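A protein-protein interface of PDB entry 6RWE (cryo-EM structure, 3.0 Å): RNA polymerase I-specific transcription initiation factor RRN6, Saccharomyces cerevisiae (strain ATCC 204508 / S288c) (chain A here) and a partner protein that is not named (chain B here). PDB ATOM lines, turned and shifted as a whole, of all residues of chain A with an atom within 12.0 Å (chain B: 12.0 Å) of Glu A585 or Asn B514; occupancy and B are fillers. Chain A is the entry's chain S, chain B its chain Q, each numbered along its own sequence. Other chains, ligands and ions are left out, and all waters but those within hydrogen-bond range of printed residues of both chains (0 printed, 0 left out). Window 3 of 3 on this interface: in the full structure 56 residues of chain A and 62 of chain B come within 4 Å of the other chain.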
ATOM      1  N   PHE A 578     -20.328   0.522 -14.395  1.00  0.00           N
ATOM      2  CA  PHE A 578     -19.156   0.084 -15.131  1.00  0.00           C
ATOM      3  C   PHE A 578     -19.430  -1.208 -15.892  1.00  0.00           C
ATOM      4  O   PHE A 578     -20.564  -1.693 -15.963  1.00  0.00           O
ATOM      5  CB  PHE A 578     -17.979  -0.119 -14.184  1.00  0.00           C
ATOM      6  CG  PHE A 578     -17.504   1.140 -13.534  1.00  0.00           C
ATOM      7  CD1 PHE A 578     -16.688   2.024 -14.222  1.00  0.00           C
ATOM      8  CD2 PHE A 578     -17.858   1.434 -12.228  1.00  0.00           C
ATOM      9  CE1 PHE A 578     -16.242   3.185 -13.624  1.00  0.00           C
ATOM     10  CE2 PHE A 578     -17.413   2.587 -11.621  1.00  0.00           C
ATOM     11  CZ  PHE A 578     -16.606   3.468 -12.323  1.00  0.00           C
ATOM     12  N   ASN A 579     -18.346  -1.758 -16.458  1.00  0.00           N
ATOM     13  CA  ASN A 579     -18.305  -3.023 -17.187  1.00  0.00           C
ATOM     14  C   ASN A 579     -19.273  -3.020 -18.363  1.00  0.00           C
ATOM     15  O   ASN A 579     -20.263  -3.759 -18.367  1.00  0.00           O
ATOM     16  CB  ASN A 579     -18.574  -4.201 -16.245  1.00  0.00           C
ATOM     17  CG  ASN A 579     -17.421  -4.453 -15.285  1.00  0.00           C
ATOM     18  OD1 ASN A 579     -16.255  -4.415 -15.677  1.00  0.00           O
ATOM     19  ND2 ASN A 579     -17.742  -4.705 -14.021  1.00  0.00           N
ATOM     20  N   ASN A 580     -19.002  -2.167 -19.349  1.00  0.00           N
ATOM     21  CA  ASN A 580     -19.890  -1.995 -20.488  1.00  0.00           C
ATOM     22  C   ASN A 580     -19.858  -3.223 -21.401  1.00  0.00           C
ATOM     23  O   ASN A 580     -19.033  -4.130 -21.259  1.00  0.00           O
ATOM     24  CB  ASN A 580     -19.505  -0.744 -21.279  1.00  0.00           C
ATOM     25  CG  ASN A 580     -19.684   0.534 -20.478  1.00  0.00           C
ATOM     26  OD1 ASN A 580     -18.711   1.206 -20.137  1.00  0.00           O
ATOM     27  ND2 ASN A 580     -20.933   0.882 -20.186  1.00  0.00           N
ATOM     28  N   ALA A 581     -20.775  -3.228 -22.365  1.00  0.00           N
ATOM     29  CA  ALA A 581     -20.932  -4.323 -23.320  1.00  0.00           C
ATOM     30  C   ALA A 581     -20.325  -3.984 -24.673  1.00  0.00           C
ATOM     31  O   ALA A 581     -20.879  -4.331 -25.721  1.00  0.00           O
ATOM     32  CB  ALA A 581     -22.407  -4.686 -23.469  1.00  0.00           C
ATOM     33  N   ASP A 582     -19.190  -3.291 -24.679  1.00  0.00           N
ATOM     34  CA  ASP A 582     -18.501  -2.917 -25.911  1.00  0.00           C
ATOM     35  C   ASP A 582     -17.312  -3.851 -26.101  1.00  0.00           C
ATOM     36  O   ASP A 582     -16.286  -3.710 -25.433  1.00  0.00           O
ATOM     37  CB  ASP A 582     -18.065  -1.457 -25.873  1.00  0.00           C
ATOM     38  CG  ASP A 582     -19.235  -0.496 -25.957  1.00  0.00           C
ATOM     39  OD1 ASP A 582     -20.266  -0.860 -26.563  1.00  0.00           O
ATOM     40  OD2 ASP A 582     -19.122   0.626 -25.421  1.00  0.00           O
ATOM     41  N   GLU A 583     -17.452  -4.801 -27.029  1.00  0.00           N
ATOM     42  CA  GLU A 583     -16.334  -5.667 -27.382  1.00  0.00           C
ATOM     43  C   GLU A 583     -15.277  -4.936 -28.199  1.00  0.00           C
ATOM     44  O   GLU A 583     -14.162  -5.447 -28.347  1.00  0.00           O
ATOM     45  CB  GLU A 583     -16.823  -6.895 -28.152  1.00  0.00           C
ATOM     46  CG  GLU A 583     -17.596  -7.905 -27.313  1.00  0.00           C
ATOM     47  CD  GLU A 583     -19.078  -7.596 -27.219  1.00  0.00           C
ATOM     48  OE1 GLU A 583     -19.532  -6.631 -27.870  1.00  0.00           O
ATOM     49  OE2 GLU A 583     -19.791  -8.323 -26.496  1.00  0.00           O
ATOM     50  N   ARG A 584     -15.609  -3.762 -28.740  1.00  0.00           N
ATOM     51  CA  ARG A 584     -14.618  -2.946 -29.432  1.00  0.00           C
ATOM     52  C   ARG A 584     -13.600  -2.377 -28.452  1.00  0.00           C
ATOM     53  O   ARG A 584     -12.388  -2.500 -28.659  1.00  0.00           O
ATOM     54  CB  ARG A 584     -15.321  -1.829 -30.201  1.00  0.00           C
ATOM     55  CG  ARG A 584     -14.390  -0.908 -30.958  1.00  0.00           C
ATOM     56  CD  ARG A 584     -13.670  -1.653 -32.069  1.00  0.00           C
ATOM     57  NE  ARG A 584     -12.820  -0.767 -32.854  1.00  0.00           N
ATOM     58  CZ  ARG A 584     -11.577  -0.441 -32.525  1.00  0.00           C
ATOM     59  NH1 ARG A 584     -11.031  -0.927 -31.418  1.00  0.00           N
ATOM     60  NH2 ARG A 584     -10.877   0.372 -33.304  1.00  0.00           N
ATOM     61  N   GLU A 585     -14.076  -1.757 -27.369  1.00  0.00           N
ATOM     62  CA  GLU A 585     -13.218  -1.235 -26.313  1.00  0.00           C
ATOM     63  C   GLU A 585     -13.011  -2.240 -25.189  1.00  0.00           C
ATOM     64  O   GLU A 585     -12.724  -1.847 -24.052  1.00  0.00           O
ATOM     65  CB  GLU A 585     -13.781   0.070 -25.749  1.00  0.00           C
ATOM     66  CG  GLU A 585     -13.719   1.249 -26.704  1.00  0.00           C
ATOM     67  CD  GLU A 585     -14.921   1.328 -27.623  1.00  0.00           C
ATOM     68  OE1 GLU A 585     -15.860   0.519 -27.456  1.00  0.00           O
ATOM     69  OE2 GLU A 585     -14.922   2.200 -28.516  1.00  0.00           O
ATOM     70  N   LYS A 586     -13.162  -3.533 -25.490  1.00  0.00           N
ATOM     71  CA  LYS A 586     -12.947  -4.576 -24.494  1.00  0.00           C
ATOM     72  C   LYS A 586     -11.483  -4.656 -24.084  1.00  0.00           C
ATOM     73  O   LYS A 586     -11.176  -4.988 -22.934  1.00  0.00           O
ATOM     74  CB  LYS A 586     -13.428  -5.914 -25.056  1.00  0.00           C
ATOM     75  CG  LYS A 586     -13.479  -7.072 -24.078  1.00  0.00           C
ATOM     76  CD  LYS A 586     -14.083  -8.294 -24.757  1.00  0.00           C
ATOM     77  CE  LYS A 586     -14.196  -9.480 -23.815  1.00  0.00           C
ATOM     78  NZ  LYS A 586     -14.800 -10.655 -24.504  1.00  0.00           N
ATOM     79  N   GLU A 587     -10.576  -4.330 -25.002  1.00  0.00           N
ATOM     80  CA  GLU A 587      -9.147  -4.308 -24.737  1.00  0.00           C
ATOM     81  C   GLU A 587      -8.546  -2.915 -24.863  1.00  0.00           C
ATOM     82  O   GLU A 587      -7.358  -2.740 -24.570  1.00  0.00           O
ATOM     83  CB  GLU A 587      -8.423  -5.273 -25.685  1.00  0.00           C
ATOM     84  CG  GLU A 587      -8.479  -4.872 -27.155  1.00  0.00           C
ATOM     85  CD  GLU A 587      -9.685  -5.444 -27.885  1.00  0.00           C
ATOM     86  OE1 GLU A 587     -10.621  -5.930 -27.217  1.00  0.00           O
ATOM     87  OE2 GLU A 587      -9.696  -5.404 -29.134  1.00  0.00           O
ATOM     88  N   SER A 588      -9.331  -1.926 -25.297  1.00  0.00           N
ATOM     89  CA  SER A 588      -8.854  -0.547 -25.347  1.00  0.00           C
ATOM     90  C   SER A 588      -8.647   0.027 -23.955  1.00  0.00           C
ATOM     91  O   SER A 588      -7.723   0.821 -23.745  1.00  0.00           O
ATOM     92  CB  SER A 588      -9.838   0.322 -26.129  1.00  0.00           C
ATOM     93  OG  SER A 588      -9.444   1.681 -26.112  1.00  0.00           O
ATOM     94  N   ILE A 589      -9.496  -0.361 -23.006  1.00  0.00           N
ATOM     95  CA  ILE A 589      -9.266  -0.025 -21.608  1.00  0.00           C
ATOM     96  C   ILE A 589      -8.077  -0.812 -21.077  1.00  0.00           C
ATOM     97  O   ILE A 589      -7.271  -0.298 -20.291  1.00  0.00           O
ATOM     98  CB  ILE A 589     -10.547  -0.301 -20.802  1.00  0.00           C
ATOM     99  CG1 ILE A 589     -11.727   0.451 -21.418  1.00  0.00           C
ATOM    100  CG2 ILE A 589     -10.380   0.117 -19.347  1.00  0.00           C
ATOM    101  CD1 ILE A 589     -13.074   0.004 -20.891  1.00  0.00           C
ATOM    102  N   GLY A 590      -7.930  -2.057 -21.530  1.00  0.00           N
ATOM    103  CA  GLY A 590      -6.813  -2.894 -21.143  1.00  0.00           C
ATOM    104  C   GLY A 590      -5.485  -2.495 -21.748  1.00  0.00           C
ATOM    105  O   GLY A 590      -4.451  -2.995 -21.295  1.00  0.00           O
ATOM    106  N   ALA A 591      -5.490  -1.617 -22.755  1.00  0.00           N
ATOM    107  CA  ALA A 591      -4.244  -1.105 -23.314  1.00  0.00           C
ATOM    108  C   ALA A 591      -3.480  -0.258 -22.306  1.00  0.00           C
ATOM    109  O   ALA A 591      -2.246  -0.209 -22.348  1.00  0.00           O
ATOM    110  CB  ALA A 591      -4.529  -0.291 -24.576  1.00  0.00           C
ATOM    111  N   LEU A 592      -4.189   0.418 -21.403  1.00  0.00           N
ATOM    112  CA  LEU A 592      -3.520   1.074 -20.291  1.00  0.00           C
ATOM    113  C   LEU A 592      -3.258   0.097 -19.155  1.00  0.00           C
ATOM    114  O   LEU A 592      -2.307   0.283 -18.388  1.00  0.00           O
ATOM    115  CB  LEU A 592      -4.351   2.265 -19.811  1.00  0.00           C
ATOM    116  CG  LEU A 592      -3.740   3.272 -18.832  1.00  0.00           C
ATOM    117  CD1 LEU A 592      -4.290   4.622 -19.159  1.00  0.00           C
ATOM    118  CD2 LEU A 592      -4.063   2.951 -17.378  1.00  0.00           C
ATOM    119  N   VAL A 593      -4.098  -0.930 -19.023  1.00  0.00           N
ATOM    120  CA  VAL A 593      -3.834  -1.978 -18.046  1.00  0.00           C
ATOM    121  C   VAL A 593      -2.604  -2.775 -18.460  1.00  0.00           C
ATOM    122  O   VAL A 593      -1.771  -3.141 -17.625  1.00  0.00           O
ATOM    123  CB  VAL A 593      -5.078  -2.871 -17.881  1.00  0.00           C
ATOM    124  CG1 VAL A 593      -4.835  -3.983 -16.872  1.00  0.00           C
ATOM    125  CG2 VAL A 593      -6.278  -2.035 -17.475  1.00  0.00           C
ATOM    126  N   SER A 594      -2.445  -3.013 -19.764  1.00  0.00           N
ATOM    127  CA  SER A 594      -1.216  -3.618 -20.256  1.00  0.00           C
ATOM    128  C   SER A 594      -0.062  -2.629 -20.279  1.00  0.00           C
ATOM    129  O   SER A 594       1.094  -3.054 -20.378  1.00  0.00           O
ATOM    130  CB  SER A 594      -1.419  -4.184 -21.659  1.00  0.00           C
ATOM    131  OG  SER A 594      -1.617  -3.142 -22.597  1.00  0.00           O
ATOM    132  N   PHE B 276      -1.766  10.095 -17.696  1.00  0.00           N
ATOM    133  CA  PHE B 276      -2.234   9.768 -19.040  1.00  0.00           C
ATOM    134  C   PHE B 276      -3.425  10.628 -19.437  1.00  0.00           C
ATOM    135  O   PHE B 276      -3.490  11.127 -20.565  1.00  0.00           O
ATOM    136  CB  PHE B 276      -2.602   8.291 -19.140  1.00  0.00           C
ATOM    137  CG  PHE B 276      -3.041   7.875 -20.513  1.00  0.00           C
ATOM    138  CD1 PHE B 276      -2.105   7.648 -21.509  1.00  0.00           C
ATOM    139  CD2 PHE B 276      -4.390   7.737 -20.821  1.00  0.00           C
ATOM    140  CE1 PHE B 276      -2.503   7.271 -22.779  1.00  0.00           C
ATOM    141  CE2 PHE B 276      -4.793   7.358 -22.084  1.00  0.00           C
ATOM    142  CZ  PHE B 276      -3.849   7.128 -23.066  1.00  0.00           C
ATOM    143  N   GLU B 277      -4.377  10.811 -18.528  1.00  0.00           N
ATOM    144  CA  GLU B 277      -5.565  11.617 -18.786  1.00  0.00           C
ATOM    145  C   GLU B 277      -5.407  12.917 -18.002  1.00  0.00           C
ATOM    146  O   GLU B 277      -5.838  13.030 -16.851  1.00  0.00           O
ATOM    147  CB  GLU B 277      -6.852  10.862 -18.415  1.00  0.00           C
ATOM    148  CG  GLU B 277      -8.161  11.652 -18.588  1.00  0.00           C
ATOM    149  CD  GLU B 277      -8.461  12.061 -20.020  1.00  0.00           C
ATOM    150  OE1 GLU B 277      -8.046  11.352 -20.953  1.00  0.00           O
ATOM    151  OE2 GLU B 277      -9.110  13.109 -20.211  1.00  0.00           O
ATOM    152  N   TRP B 316     -10.108  -0.319 -11.835  1.00  0.00           N
ATOM    153  CA  TRP B 316      -9.474  -0.980 -12.972  1.00  0.00           C
ATOM    154  C   TRP B 316      -8.328  -1.884 -12.546  1.00  0.00           C
ATOM    155  O   TRP B 316      -8.097  -2.927 -13.167  1.00  0.00           O
ATOM    156  CB  TRP B 316      -8.976   0.068 -13.954  1.00  0.00           C
ATOM    157  CG  TRP B 316     -10.070   0.764 -14.663  1.00  0.00           C
ATOM    158  CD1 TRP B 316     -11.372   0.373 -14.748  1.00  0.00           C
ATOM    159  CD2 TRP B 316      -9.974   2.005 -15.356  1.00  0.00           C
ATOM    160  NE1 TRP B 316     -12.089   1.284 -15.480  1.00  0.00           N
ATOM    161  CE2 TRP B 316     -11.253   2.298 -15.863  1.00  0.00           C
ATOM    162  CE3 TRP B 316      -8.926   2.891 -15.611  1.00  0.00           C
ATOM    163  CZ2 TRP B 316     -11.512   3.444 -16.608  1.00  0.00           C
ATOM    164  CZ3 TRP B 316      -9.183   4.026 -16.348  1.00  0.00           C
ATOM    165  CH2 TRP B 316     -10.465   4.293 -16.840  1.00  0.00           C
ATOM    166  N   SER B 319     -10.283  -5.054 -11.173  1.00  0.00           N
ATOM    167  CA  SER B 319     -11.164  -5.711 -12.133  1.00  0.00           C
ATOM    168  C   SER B 319     -10.365  -6.380 -13.243  1.00  0.00           C
ATOM    169  O   SER B 319     -10.558  -7.567 -13.533  1.00  0.00           O
ATOM    170  CB  SER B 319     -12.149  -4.696 -12.715  1.00  0.00           C
ATOM    171  OG  SER B 319     -12.971  -5.280 -13.708  1.00  0.00           O
ATOM    172  N   PHE B 320      -9.468  -5.633 -13.884  1.00  0.00           N
ATOM    173  CA  PHE B 320      -8.635  -6.179 -14.956  1.00  0.00           C
ATOM    174  C   PHE B 320      -7.311  -6.663 -14.366  1.00  0.00           C
ATOM    175  O   PHE B 320      -6.239  -6.095 -14.580  1.00  0.00           O
ATOM    176  CB  PHE B 320      -8.420  -5.142 -16.051  1.00  0.00           C
ATOM    177  CG  PHE B 320      -9.641  -4.872 -16.891  1.00  0.00           C
ATOM    178  CD1 PHE B 320     -10.729  -5.734 -16.874  1.00  0.00           C
ATOM    179  CD2 PHE B 320      -9.694  -3.756 -17.708  1.00  0.00           C
ATOM    180  CE1 PHE B 320     -11.846  -5.481 -17.647  1.00  0.00           C
ATOM    181  CE2 PHE B 320     -10.805  -3.499 -18.484  1.00  0.00           C
ATOM    182  CZ  PHE B 320     -11.881  -4.362 -18.453  1.00  0.00           C
ATOM    183  N   ILE B 505     -15.207  12.247 -16.406  1.00  0.00           N
ATOM    184  CA  ILE B 505     -13.840  11.737 -16.436  1.00  0.00           C
ATOM    185  C   ILE B 505     -13.755  10.450 -17.241  1.00  0.00           C
ATOM    186  O   ILE B 505     -12.858  10.292 -18.080  1.00  0.00           O
ATOM    187  CB  ILE B 505     -13.309  11.562 -15.002  1.00  0.00           C
ATOM    188  CG1 ILE B 505     -13.044  12.934 -14.373  1.00  0.00           C
ATOM    189  CG2 ILE B 505     -12.101  10.631 -14.945  1.00  0.00           C
ATOM    190  CD1 ILE B 505     -12.107  13.811 -15.168  1.00  0.00           C
ATOM    191  N   LYS B 506     -14.682   9.516 -17.015  1.00  0.00           N
ATOM    192  CA  LYS B 506     -14.688   8.241 -17.725  1.00  0.00           C
ATOM    193  C   LYS B 506     -14.920   8.406 -19.219  1.00  0.00           C
ATOM    194  O   LYS B 506     -14.190   7.818 -20.022  1.00  0.00           O
ATOM    195  CB  LYS B 506     -15.754   7.305 -17.152  1.00  0.00           C
ATOM    196  CG  LYS B 506     -15.806   5.951 -17.842  1.00  0.00           C
ATOM    197  CD  LYS B 506     -16.882   5.060 -17.249  1.00  0.00           C
ATOM    198  CE  LYS B 506     -16.970   3.740 -17.994  1.00  0.00           C
ATOM    199  NZ  LYS B 506     -17.995   2.843 -17.401  1.00  0.00           N
ATOM    200  N   ASN B 507     -15.907   9.208 -19.613  1.00  0.00           N
ATOM    201  CA  ASN B 507     -16.089   9.509 -21.030  1.00  0.00           C
ATOM    202  C   ASN B 507     -15.317  10.746 -21.466  1.00  0.00           C
ATOM    203  O   ASN B 507     -15.847  11.620 -22.154  1.00  0.00           O
ATOM    204  CB  ASN B 507     -17.577   9.661 -21.321  1.00  0.00           C
ATOM    205  CG  ASN B 507     -18.354   8.408 -20.997  1.00  0.00           C
ATOM    206  OD1 ASN B 507     -19.214   8.409 -20.119  1.00  0.00           O
ATOM    207  ND2 ASN B 507     -18.035   7.320 -21.685  1.00  0.00           N
ATOM    208  N   ALA B 508     -14.055  10.830 -21.056  1.00  0.00           N
ATOM    209  CA  ALA B 508     -13.065  11.717 -21.642  1.00  0.00           C
ATOM    210  C   ALA B 508     -11.750  10.954 -21.702  1.00  0.00           C
ATOM    211  O   ALA B 508     -10.811  11.357 -22.395  1.00  0.00           O
ATOM    212  CB  ALA B 508     -12.932  13.004 -20.829  1.00  0.00           C
ATOM    213  N   CYS B 509     -11.690   9.836 -20.972  1.00  0.00           N
ATOM    214  CA  CYS B 509     -10.472   9.050 -20.826  1.00  0.00           C
ATOM    215  C   CYS B 509     -10.369   7.912 -21.827  1.00  0.00           C
ATOM    216  O   CYS B 509      -9.270   7.645 -22.327  1.00  0.00           O
ATOM    217  CB  CYS B 509     -10.379   8.477 -19.406  1.00  0.00           C
ATOM    218  SG  CYS B 509      -8.880   7.520 -19.067  1.00  0.00           S
ATOM    219  N   LEU B 510     -11.481   7.248 -22.146  1.00  0.00           N
ATOM    220  CA  LEU B 510     -11.480   6.276 -23.231  1.00  0.00           C
ATOM    221  C   LEU B 510     -11.374   6.941 -24.592  1.00  0.00           C
ATOM    222  O   LEU B 510     -10.993   6.279 -25.563  1.00  0.00           O
ATOM    223  CB  LEU B 510     -12.737   5.404 -23.183  1.00  0.00           C
ATOM    224  CG  LEU B 510     -12.757   4.178 -22.263  1.00  0.00           C
ATOM    225  CD1 LEU B 510     -12.899   4.541 -20.789  1.00  0.00           C
ATOM    226  CD2 LEU B 510     -13.872   3.241 -22.692  1.00  0.00           C
ATOM    227  N   HIS B 511     -11.663   8.242 -24.671  1.00  0.00           N
ATOM    228  CA  HIS B 511     -11.552   9.042 -25.884  1.00  0.00           C
ATOM    229  C   HIS B 511     -10.104   9.253 -26.324  1.00  0.00           C
ATOM    230  O   HIS B 511      -9.873   9.752 -27.430  1.00  0.00           O
ATOM    231  CB  HIS B 511     -12.248  10.387 -25.641  1.00  0.00           C
ATOM    232  CG  HIS B 511     -12.495  11.192 -26.877  1.00  0.00           C
ATOM    233  ND1 HIS B 511     -11.562  12.064 -27.396  1.00  0.00           N
ATOM    234  CD2 HIS B 511     -13.574  11.268 -27.690  1.00  0.00           C
ATOM    235  CE1 HIS B 511     -12.056  12.639 -28.480  1.00  0.00           C
ATOM    236  NE2 HIS B 511     -13.275  12.172 -28.680  1.00  0.00           N
ATOM    237  N   ARG B 512      -9.126   8.871 -25.495  1.00  0.00           N
ATOM    238  CA  ARG B 512      -7.727   8.949 -25.900  1.00  0.00           C
ATOM    239  C   ARG B 512      -7.406   7.913 -26.968  1.00  0.00           C
ATOM    240  O   ARG B 512      -6.730   8.217 -27.958  1.00  0.00           O
ATOM    241  CB  ARG B 512      -6.819   8.757 -24.686  1.00  0.00           C
ATOM    242  CG  ARG B 512      -7.034   9.787 -23.605  1.00  0.00           C
ATOM    243  CD  ARG B 512      -6.707  11.182 -24.108  1.00  0.00           C
ATOM    244  NE  ARG B 512      -5.304  11.328 -24.483  1.00  0.00           N
ATOM    245  CZ  ARG B 512      -4.348  11.719 -23.648  1.00  0.00           C
ATOM    246  NH1 ARG B 512      -4.648  12.015 -22.392  1.00  0.00           N
ATOM    247  NH2 ARG B 512      -3.097  11.828 -24.073  1.00  0.00           N
ATOM    248  N   MET B 513      -7.879   6.683 -26.784  1.00  0.00           N
ATOM    249  CA  MET B 513      -7.657   5.654 -27.791  1.00  0.00           C
ATOM    250  C   MET B 513      -8.658   5.779 -28.935  1.00  0.00           C
ATOM    251  O   MET B 513      -8.329   5.494 -30.091  1.00  0.00           O
ATOM    252  CB  MET B 513      -7.721   4.272 -27.144  1.00  0.00           C
ATOM    253  CG  MET B 513      -6.450   3.889 -26.396  1.00  0.00           C
ATOM    254  SD  MET B 513      -6.208   4.844 -24.887  1.00  0.00           S
ATOM    255  CE  MET B 513      -7.471   4.135 -23.835  1.00  0.00           C
ATOM    256  N   ASN B 514      -9.883   6.199 -28.630  1.00  0.00           N
ATOM    257  CA  ASN B 514     -10.862   6.518 -29.663  1.00  0.00           C
ATOM    258  C   ASN B 514     -11.828   7.619 -29.225  1.00  0.00           C
ATOM    259  O   ASN B 514     -11.669   8.781 -29.597  1.00  0.00           O
ATOM    260  CB  ASN B 514     -11.631   5.259 -30.088  1.00  0.00           C
ATOM    261  CG  ASN B 514     -12.310   4.544 -28.926  1.00  0.00           C
ATOM    262  OD1 ASN B 514     -12.282   4.993 -27.782  1.00  0.00           O
ATOM    263  ND2 ASN B 514     -12.928   3.409 -29.228  1.00  0.00           N
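O of Leu B510 sits close to OD1 of Asn B514.
Of the 17 printed residues of chain A, 8 touch a printed residue of chain B.
Among the printed residues, 9 pairs touch across the chains.
The side-chain amide nitrogen of Asn B514 sits at hydrogen-bond distance from the side-chain carboxylate of Glu A585 (2.4 Å).
The side-chain amino group (NZ) of Lys B506 lies within hydrogen-bond range of the side-chain amide oxygen (OD1) of Asn A580.
Of the printed residues of chain B, Phe A578 touches Lys B506.
No residue of chain B comes within 4 Å of Asp A582.
No residue of chain B comes within 4 Å of Arg A584.
Glu A585 touches just one residue of chain B: Asn B514 (2.4 Å).
Ile A589 touches two residues of chain B.
Trp B316 touches none of the printed residues of chain A.
Printed residues of chain A within 4 Å of Lys B506: Phe A578 (3.5 Å) and Asn A580 (3.3 Å).
Ala B508 touches none of the printed residues of chain A.
No residue of chain A comes within 4 Å of His B511.
Of the printed residues of chain A, Met B513 touches Ser A588.
Of the printed residues of chain A, Asn B514 touches Glu A585.
The nearest residue of chain B that does not touch Glu A585 is Leu B510 (4.4 Å).
The nearest printed residue of chain A that does not touch Lys B506 is Asn A579 (4.7 Å).
Among the printed residues, pairs that only touch across the chains: Ser A588 with Met B513, Val A593 with Phe B320, Leu A592 with Phe B276, Phe A578 with Lys B506, Ile A589 with Phe B320, Ile A589 with Leu B510 and Asn A579 with Ser B319.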
